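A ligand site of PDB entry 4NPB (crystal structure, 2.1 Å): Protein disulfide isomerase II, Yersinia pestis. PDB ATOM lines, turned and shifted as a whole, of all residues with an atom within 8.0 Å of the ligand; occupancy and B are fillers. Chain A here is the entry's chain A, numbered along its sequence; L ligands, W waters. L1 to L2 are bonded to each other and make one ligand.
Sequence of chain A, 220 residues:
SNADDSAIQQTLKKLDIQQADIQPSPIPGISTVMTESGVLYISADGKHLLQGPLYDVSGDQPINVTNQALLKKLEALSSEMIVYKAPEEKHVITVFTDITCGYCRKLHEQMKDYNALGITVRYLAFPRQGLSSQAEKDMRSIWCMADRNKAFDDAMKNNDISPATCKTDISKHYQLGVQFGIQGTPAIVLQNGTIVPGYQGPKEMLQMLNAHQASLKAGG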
ATOM      1  N   LEU A  77       0.175  -2.738  -6.920  1.00  0.00           N
ATOM      2  CA  LEU A  77      -0.637  -2.073  -5.886  1.00  0.00           C
ATOM      3  C   LEU A  77      -1.988  -1.556  -6.389  1.00  0.00           C
ATOM      4  O   LEU A  77      -2.689  -0.850  -5.661  1.00  0.00           O
ATOM      5  CB  LEU A  77       0.150  -0.928  -5.280  1.00  0.00           C
ATOM      6  CG  LEU A  77       1.405  -1.282  -4.505  1.00  0.00           C
ATOM      7  CD1 LEU A  77       2.121  -0.005  -4.128  1.00  0.00           C
ATOM      8  CD2 LEU A  77       1.059  -2.074  -3.257  1.00  0.00           C
ATOM      9  N   SER A  78      -2.357  -1.896  -7.627  1.00  0.00           N
ATOM     10  CA  SER A  78      -3.569  -1.357  -8.245  1.00  0.00           C
ATOM     11  C   SER A  78      -4.826  -1.555  -7.374  1.00  0.00           C
ATOM     12  O   SER A  78      -5.662  -0.659  -7.305  1.00  0.00           O
ATOM     13  CB  SER A  78      -3.778  -1.952  -9.640  1.00  0.00           C
ATOM     14  OG  SER A  78      -3.942  -3.358  -9.565  1.00  0.00           O
ATOM     15  N   SER A  79      -4.940  -2.691  -6.694  1.00  0.00           N
ATOM     16  CA  SER A  79      -6.092  -2.929  -5.799  1.00  0.00           C
ATOM     17  C   SER A  79      -6.084  -2.028  -4.562  1.00  0.00           C
ATOM     18  O   SER A  79      -7.097  -1.925  -3.838  1.00  0.00           O
ATOM     19  CB  SER A  79      -6.166  -4.394  -5.372  1.00  0.00           C
ATOM     20  OG  SER A  79      -5.105  -4.734  -4.499  1.00  0.00           O
ATOM     21  N   GLU A  80      -4.957  -1.365  -4.301  1.00  0.00           N
ATOM     22  CA  GLU A  80      -4.842  -0.477  -3.135  1.00  0.00           C
ATOM     23  C   GLU A  80      -5.077   0.972  -3.509  1.00  0.00           C
ATOM     24  O   GLU A  80      -5.016   1.858  -2.662  1.00  0.00           O
ATOM     25  CB  GLU A  80      -3.458  -0.591  -2.499  1.00  0.00           C
ATOM     26  CG  GLU A  80      -2.985  -2.011  -2.250  1.00  0.00           C
ATOM     27  CD  GLU A  80      -4.003  -2.787  -1.443  1.00  0.00           C
ATOM     28  OE1 GLU A  80      -4.543  -3.796  -1.959  1.00  0.00           O
ATOM     29  OE2 GLU A  80      -4.276  -2.375  -0.303  1.00  0.00           O
ATOM     30  N   MET A  81      -5.330   1.224  -4.793  1.00  0.00           N
ATOM     31  CA  MET A  81      -5.461   2.596  -5.279  1.00  0.00           C
ATOM     32  C   MET A  81      -6.865   3.142  -5.131  1.00  0.00           C
ATOM     33  O   MET A  81      -7.854   2.396  -5.209  1.00  0.00           O
ATOM     34  CB  MET A  81      -5.049   2.677  -6.748  1.00  0.00           C
ATOM     35  CG  MET A  81      -3.564   2.442  -6.959  1.00  0.00           C
ATOM     36  SD  MET A  81      -3.060   2.347  -8.861  1.00  0.00           S
ATOM     37  CE  MET A  81      -1.176   1.943  -8.465  1.00  0.00           C
ATOM     38  N   ILE A  82      -6.953   4.448  -4.923  1.00  0.00           N
ATOM     39  CA  ILE A  82      -8.238   5.126  -4.950  1.00  0.00           C
ATOM     40  C   ILE A  82      -8.399   5.634  -6.378  1.00  0.00           C
ATOM     41  O   ILE A  82      -7.667   6.514  -6.808  1.00  0.00           O
ATOM     42  CB  ILE A  82      -8.284   6.284  -3.940  1.00  0.00           C
ATOM     43  CG1 ILE A  82      -7.971   5.772  -2.529  1.00  0.00           C
ATOM     44  CG2 ILE A  82      -9.642   6.977  -3.995  1.00  0.00           C
ATOM     45  CD1 ILE A  82      -8.175   6.808  -1.432  1.00  0.00           C
ATOM     46  N   ARG A 140      -3.881   6.212   6.324  1.00  0.00           N
ATOM     47  CA  ARG A 140      -4.106   4.796   6.633  1.00  0.00           C
ATOM     48  C   ARG A 140      -5.605   4.582   6.868  1.00  0.00           C
ATOM     49  O   ARG A 140      -6.197   3.635   6.362  1.00  0.00           O
ATOM     50  CB  ARG A 140      -3.345   4.363   7.876  1.00  0.00           C
ATOM     51  CG  ARG A 140      -3.538   2.899   8.250  1.00  0.00           C
ATOM     52  CD  ARG A 140      -4.256   2.804   9.593  1.00  0.00           C
ATOM     53  NE  ARG A 140      -3.446   3.317  10.702  1.00  0.00           N
ATOM     54  CZ  ARG A 140      -3.930   4.049  11.708  1.00  0.00           C
ATOM     55  NH1 ARG A 140      -3.138   4.481  12.679  1.00  0.00           N
ATOM     56  NH2 ARG A 140      -5.222   4.357  11.728  1.00  0.00           N
ATOM     57  N   SER A 141      -6.189   5.505   7.633  1.00  0.00           N
ATOM     58  CA  SER A 141      -7.608   5.441   7.963  1.00  0.00           C
ATOM     59  C   SER A 141      -8.471   5.503   6.692  1.00  0.00           C
ATOM     60  O   SER A 141      -9.385   4.673   6.514  1.00  0.00           O
ATOM     61  CB  SER A 141      -7.983   6.565   8.935  1.00  0.00           C
ATOM     62  OG  SER A 141      -7.435   6.310  10.205  1.00  0.00           O
ATOM     63  N   ILE A 142      -8.160   6.449   5.809  1.00  0.00           N
ATOM     64  CA  ILE A 142      -8.854   6.580   4.534  1.00  0.00           C
ATOM     65  C   ILE A 142      -8.807   5.298   3.696  1.00  0.00           C
ATOM     66  O   ILE A 142      -9.851   4.753   3.308  1.00  0.00           O
ATOM     67  CB  ILE A 142      -8.269   7.732   3.719  1.00  0.00           C
ATOM     68  CG1 ILE A 142      -8.650   9.065   4.377  1.00  0.00           C
ATOM     69  CG2 ILE A 142      -8.737   7.669   2.227  1.00  0.00           C
ATOM     70  CD1 ILE A 142      -7.710  10.215   3.995  1.00  0.00           C
ATOM     71  N   TRP A 143      -7.598   4.814   3.433  1.00  0.00           N
ATOM     72  CA  TRP A 143      -7.401   3.626   2.609  1.00  0.00           C
ATOM     73  C   TRP A 143      -8.018   2.348   3.177  1.00  0.00           C
ATOM     74  O   TRP A 143      -8.289   1.392   2.426  1.00  0.00           O
ATOM     75  CB  TRP A 143      -5.917   3.411   2.345  1.00  0.00           C
ATOM     76  CG  TRP A 143      -5.520   3.940   1.000  1.00  0.00           C
ATOM     77  CD1 TRP A 143      -5.360   3.223  -0.141  1.00  0.00           C
ATOM     78  CD2 TRP A 143      -5.259   5.317   0.655  1.00  0.00           C
ATOM     79  NE1 TRP A 143      -5.003   4.063  -1.193  1.00  0.00           N
ATOM     80  CE2 TRP A 143      -4.944   5.346  -0.726  1.00  0.00           C
ATOM     81  CE3 TRP A 143      -5.272   6.511   1.377  1.00  0.00           C
ATOM     82  CZ2 TRP A 143      -4.623   6.532  -1.391  1.00  0.00           C
ATOM     83  CZ3 TRP A 143      -4.979   7.694   0.711  1.00  0.00           C
ATOM     84  CH2 TRP A 143      -4.639   7.695  -0.668  1.00  0.00           C
ATOM     85  N   CYS A 144      -8.244   2.325   4.490  1.00  0.00           N
ATOM     86  CA  CYS A 144      -8.939   1.204   5.150  1.00  0.00           C
ATOM     87  C   CYS A 144     -10.461   1.203   4.978  1.00  0.00           C
ATOM     88  O   CYS A 144     -11.113   0.201   5.301  1.00  0.00           O
ATOM     89  CB  CYS A 144      -8.616   1.171   6.649  1.00  0.00           C
ATOM     90  SG  CYS A 144      -6.990   0.463   7.082  1.00  0.00           S
ATOM     91  N   MET A 145     -11.067   2.294   4.499  1.00  0.00           N
ATOM     92  CA  MET A 145     -12.538   2.306   4.418  1.00  0.00           C
ATOM     93  C   MET A 145     -13.073   1.512   3.221  1.00  0.00           C
ATOM     94  O   MET A 145     -12.457   1.525   2.133  1.00  0.00           O
ATOM     95  CB  MET A 145     -13.086   3.736   4.334  1.00  0.00           C
ATOM     96  CG  MET A 145     -12.691   4.675   5.459  1.00  0.00           C
ATOM     97  SD  MET A 145     -13.135   3.974   7.210  1.00  0.00           S
ATOM     98  CE  MET A 145     -15.059   4.343   7.260  1.00  0.00           C
ATOM     99  N   ALA A 146     -14.210   0.846   3.420  1.00  0.00           N
ATOM    100  CA  ALA A 146     -14.883   0.123   2.341  1.00  0.00           C
ATOM    101  C   ALA A 146     -15.074   0.965   1.088  1.00  0.00           C
ATOM    102  O   ALA A 146     -15.043   0.439  -0.022  1.00  0.00           O
ATOM    103  CB  ALA A 146     -16.232  -0.420   2.823  1.00  0.00           C
ATOM    104  N   ASP A 147     -15.267   2.269   1.271  1.00  0.00           N
ATOM    105  CA  ASP A 147     -15.369   3.195   0.144  1.00  0.00           C
ATOM    106  C   ASP A 147     -14.267   4.234   0.236  1.00  0.00           C
ATOM    107  O   ASP A 147     -14.462   5.299   0.835  1.00  0.00           O
ATOM    108  CB  ASP A 147     -16.738   3.897   0.141  1.00  0.00           C
ATOM    109  CG  ASP A 147     -17.012   4.681  -1.147  1.00  0.00           C
ATOM    110  OD1 ASP A 147     -16.057   4.997  -1.911  1.00  0.00           O
ATOM    111  OD2 ASP A 147     -18.192   5.013  -1.392  1.00  0.00           O
ATOM    112  N   ARG A 148     -13.116   3.937  -0.377  1.00  0.00           N
ATOM    113  CA  ARG A 148     -11.961   4.805  -0.257  1.00  0.00           C
ATOM    114  C   ARG A 148     -12.264   6.173  -0.871  1.00  0.00           C
ATOM    115  O   ARG A 148     -11.813   7.214  -0.380  1.00  0.00           O
ATOM    116  CB  ARG A 148     -10.740   4.194  -0.947  1.00  0.00           C
ATOM    117  CG  ARG A 148     -10.305   2.831  -0.415  1.00  0.00           C
ATOM    118  CD  ARG A 148      -8.886   2.547  -0.867  1.00  0.00           C
ATOM    119  NE  ARG A 148      -8.402   1.229  -0.433  1.00  0.00           N
ATOM    120  CZ  ARG A 148      -8.229   0.198  -1.243  1.00  0.00           C
ATOM    121  NH1 ARG A 148      -8.510   0.306  -2.547  1.00  0.00           N
ATOM    122  NH2 ARG A 148      -7.792  -0.961  -0.760  1.00  0.00           N
ATOM    123  N   ASN A 149     -13.038   6.144  -1.955  1.00  0.00           N
ATOM    124  CA  ASN A 149     -13.353   7.361  -2.711  1.00  0.00           C
ATOM    125  C   ASN A 149     -14.091   8.365  -1.843  1.00  0.00           C
ATOM    126  O   ASN A 149     -13.699   9.525  -1.785  1.00  0.00           O
ATOM    127  CB  ASN A 149     -14.165   7.019  -3.976  1.00  0.00           C
ATOM    128  CG  ASN A 149     -13.322   6.302  -5.040  1.00  0.00           C
ATOM    129  OD1 ASN A 149     -13.012   5.116  -4.918  1.00  0.00           O
ATOM    130  ND2 ASN A 149     -12.977   7.029  -6.099  1.00  0.00           N
ATOM    131  N   THR A 165      -8.466   1.138  11.213  1.00  0.00           N
ATOM    132  CA  THR A 165      -7.414   0.193  10.861  1.00  0.00           C
ATOM    133  C   THR A 165      -8.052  -1.000  10.142  1.00  0.00           C
ATOM    134  O   THR A 165      -9.262  -1.246  10.287  1.00  0.00           O
ATOM    135  CB  THR A 165      -6.694  -0.309  12.112  1.00  0.00           C
ATOM    136  OG1 THR A 165      -7.593  -1.102  12.891  1.00  0.00           O
ATOM    137  CG2 THR A 165      -6.224   0.867  12.959  1.00  0.00           C
ATOM    138  N   CYS A 166      -7.251  -1.750   9.401  1.00  0.00           N
ATOM    139  CA  CYS A 166      -7.747  -2.948   8.715  1.00  0.00           C
ATOM    140  C   CYS A 166      -6.631  -3.974   8.586  1.00  0.00           C
ATOM    141  O   CYS A 166      -5.840  -4.150   9.511  1.00  0.00           O
ATOM    142  CB  CYS A 166      -8.319  -2.585   7.335  1.00  0.00           C
ATOM    143  SG  CYS A 166      -7.282  -1.439   6.372  1.00  0.00           S
ATOM    144  N   LYS A 167      -6.562  -4.652   7.436  1.00  0.00           N
ATOM    145  CA  LYS A 167      -5.554  -5.686   7.202  1.00  0.00           C
ATOM    146  C   LYS A 167      -4.215  -5.092   6.773  1.00  0.00           C
ATOM    147  O   LYS A 167      -3.167  -5.690   7.009  1.00  0.00           O
ATOM    148  CB  LYS A 167      -6.014  -6.700   6.148  1.00  0.00           C
ATOM    149  CG  LYS A 167      -7.277  -7.494   6.499  1.00  0.00           C
ATOM    150  CD  LYS A 167      -7.630  -8.478   5.374  1.00  0.00           C
ATOM    151  CE  LYS A 167      -8.915  -9.244   5.665  1.00  0.00           C
ATOM    152  NZ  LYS A 167      -9.078 -10.452   4.806  1.00  0.00           N
ATOM    153  N   THR A 168      -4.258  -3.928   6.144  1.00  0.00           N
ATOM    154  CA  THR A 168      -3.034  -3.298   5.646  1.00  0.00           C
ATOM    155  C   THR A 168      -2.939  -1.822   5.977  1.00  0.00           C
ATOM    156  O   THR A 168      -3.957  -1.136   6.139  1.00  0.00           O
ATOM    157  CB  THR A 168      -2.927  -3.408   4.111  1.00  0.00           C
ATOM    158  OG1 THR A 168      -4.120  -2.860   3.517  1.00  0.00           O
ATOM    159  CG2 THR A 168      -2.729  -4.853   3.687  1.00  0.00           C
ATOM    160  N   ASP A 169      -1.704  -1.334   6.050  1.00  0.00           N
ATOM    161  CA  ASP A 169      -1.437   0.095   6.111  1.00  0.00           C
ATOM    162  C   ASP A 169      -0.952   0.570   4.738  1.00  0.00           C
ATOM    163  O   ASP A 169      -1.131  -0.131   3.734  1.00  0.00           O
ATOM    164  CB  ASP A 169      -0.413   0.418   7.206  1.00  0.00           C
ATOM    165  CG  ASP A 169       0.910  -0.342   7.031  1.00  0.00           C
ATOM    166  OD1 ASP A 169       1.375  -0.506   5.885  1.00  0.00           O
ATOM    167  OD2 ASP A 169       1.490  -0.772   8.047  1.00  0.00           O
ATOM    168  N   HIS A 173       3.070   2.066  -0.055  1.00  0.00           N
ATOM    169  CA  HIS A 173       2.878   3.186  -0.969  1.00  0.00           C
ATOM    170  C   HIS A 173       4.027   4.167  -0.800  1.00  0.00           C
ATOM    171  O   HIS A 173       4.640   4.602  -1.775  1.00  0.00           O
ATOM    172  CB  HIS A 173       1.576   3.943  -0.651  1.00  0.00           C
ATOM    173  CG  HIS A 173       0.347   3.093  -0.647  1.00  0.00           C
ATOM    174  ND1 HIS A 173      -0.907   3.622  -0.843  1.00  0.00           N
ATOM    175  CD2 HIS A 173       0.165   1.762  -0.428  1.00  0.00           C
ATOM    176  CE1 HIS A 173      -1.808   2.655  -0.765  1.00  0.00           C
ATOM    177  NE2 HIS A 173      -1.176   1.517  -0.518  1.00  0.00           N
HETATM  178  C1  LIG L   1     -10.835  -4.323   0.387  1.00  0.00           C
HETATM  179  C2  LIG L   1     -11.855  -3.815  -0.641  1.00  0.00           C
HETATM  180  C3  LIG L   1     -11.717  -2.309  -0.893  1.00  0.00           C
HETATM  181  C4  LIG L   1     -11.789  -1.583   0.439  1.00  0.00           C
HETATM  182  C5  LIG L   1     -10.739  -2.164   1.383  1.00  0.00           C
HETATM  183  C6  LIG L   1     -10.649  -1.424   2.729  1.00  0.00           C
HETATM  184  O1  LIG L   1     -11.736  -4.515  -1.852  1.00  0.00           O
HETATM  185  O2  LIG L   1     -12.696  -1.838  -1.798  1.00  0.00           O
HETATM  186  O3  LIG L   1     -11.582  -0.194   0.268  1.00  0.00           O
HETATM  187  O4  LIG L   1     -10.968  -3.559   1.573  1.00  0.00           O
HETATM  188  O5  LIG L   1     -11.870  -1.469   3.463  1.00  0.00           O
HETATM  189  C1  LG2 L   2      -8.913  -6.556  -0.393  1.00  0.00           C
HETATM  190  C2  LG2 L   2      -8.571  -5.240   0.303  1.00  0.00           C
HETATM  191  C3  LG2 L   2      -7.162  -4.748  -0.071  1.00  0.00           C
HETATM  192  C4  LG2 L   2      -6.724  -3.998   1.172  1.00  0.00           C
HETATM  193  C5  LG2 L   2      -7.434  -4.751   2.294  1.00  0.00           C
HETATM  194  C6  LG2 L   2      -7.897  -3.808   3.397  1.00  0.00           C
HETATM  195  O1  LG2 L   2      -7.929  -7.524  -0.098  1.00  0.00           O
HETATM  196  O2  LG2 L   2      -9.499  -4.223  -0.097  1.00  0.00           O
HETATM  197  O3  LG2 L   2      -7.189  -3.904  -1.190  1.00  0.00           O
HETATM  198  O4  LG2 L   2      -5.323  -3.991   1.320  1.00  0.00           O
HETATM  199  O5  LG2 L   2      -8.545  -5.407   1.719  1.00  0.00           O
HETATM  200  O6  LG2 L   2      -7.811  -4.506   4.616  1.00  0.00           O
HETATM  201  O   HOH W   1     -15.259  -1.788  -1.263  1.00  0.00           O
HETATM  202  O   HOH W   2     -11.524  -1.033  -4.178  1.00  0.00           O
HETATM  203  O   HOH W   3     -12.901   1.614  -1.911  1.00  0.00           O
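Trp 143 touches the ligand. Of the 22 residues printed, 10 come within 4 Å of the ligand.
O4 of LG2 L2 is in hydrogen-bond range of OE2 of Glu 80 (2.5 Å). An oxygen (O5) of LIG L1 lies within hydrogen-bond range of the backbone carbonyl oxygen of Cys 144, at 2.6 Å. The backbone carbonyl oxygen of Met 145 is in hydrogen-bond range of an oxygen (O3) of LIG L1 (2.7 Å). An oxygen (O4) of LG2 L2 sits at hydrogen-bond distance from the side-chain hydroxyl of Thr 168. The guanidinium group of Arg 148 sits at hydrogen-bond distance from an oxygen (O3) of LG2 L2 (3.0 Å). O6 of LG2 L2 is in hydrogen-bond range of N of Lys 167, 3.1 Å away. The backbone NH of Ala 146 is in hydrogen-bond range of an oxygen (O5) of LIG L1, 3.3 Å away. The backbone carbonyl oxygen (O) of Ser 79 is in hydrogen-bond range of an oxygen (O3) of LG2 L2 (3.3 Å). The side-chain sulfur of Cys 166 sits close to an oxygen (O6) of LG2 L2.
Water W1 bridges the backbone carbonyl oxygen (O) of Ala 146 (2.6 Å) and an oxygen (O2) of LIG L1 (2.6 Å). Water W3 lies within hydrogen-bond range of N of Arg 148 (2.8 Å), O of Ala 146 (3.1 Å) and O3 of LIG L1 (3.1 Å).
The guanidinium group of Arg 148 lies within salt-bridge range of the side-chain carboxylate of Glu 80, at 3.8 Å. OE1 of Glu 80 sits at hydrogen-bond distance from OG of Ser 79, 2.8 Å away. The backbone carbonyl oxygen (O) of Glu 80 lies within hydrogen-bond range of the indole nitrogen (NE1) of Trp 143 (2.6 Å). The side-chain sulfur (SG) of Cys 144 forms a disulfide with the side-chain sulfur (SG) of Cys 166 (2.1 Å). The guanidinium group of Arg 148 is in hydrogen-bond range of the backbone carbonyl oxygen of Ser 79 (2.9 Å). NE of Arg 148 sits at hydrogen-bond distance from O of Trp 143 (2.9 Å). The backbone carbonyl oxygen of Met 81 is in hydrogen-bond range of the guanidinium group of Arg 148 (3.4 Å).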
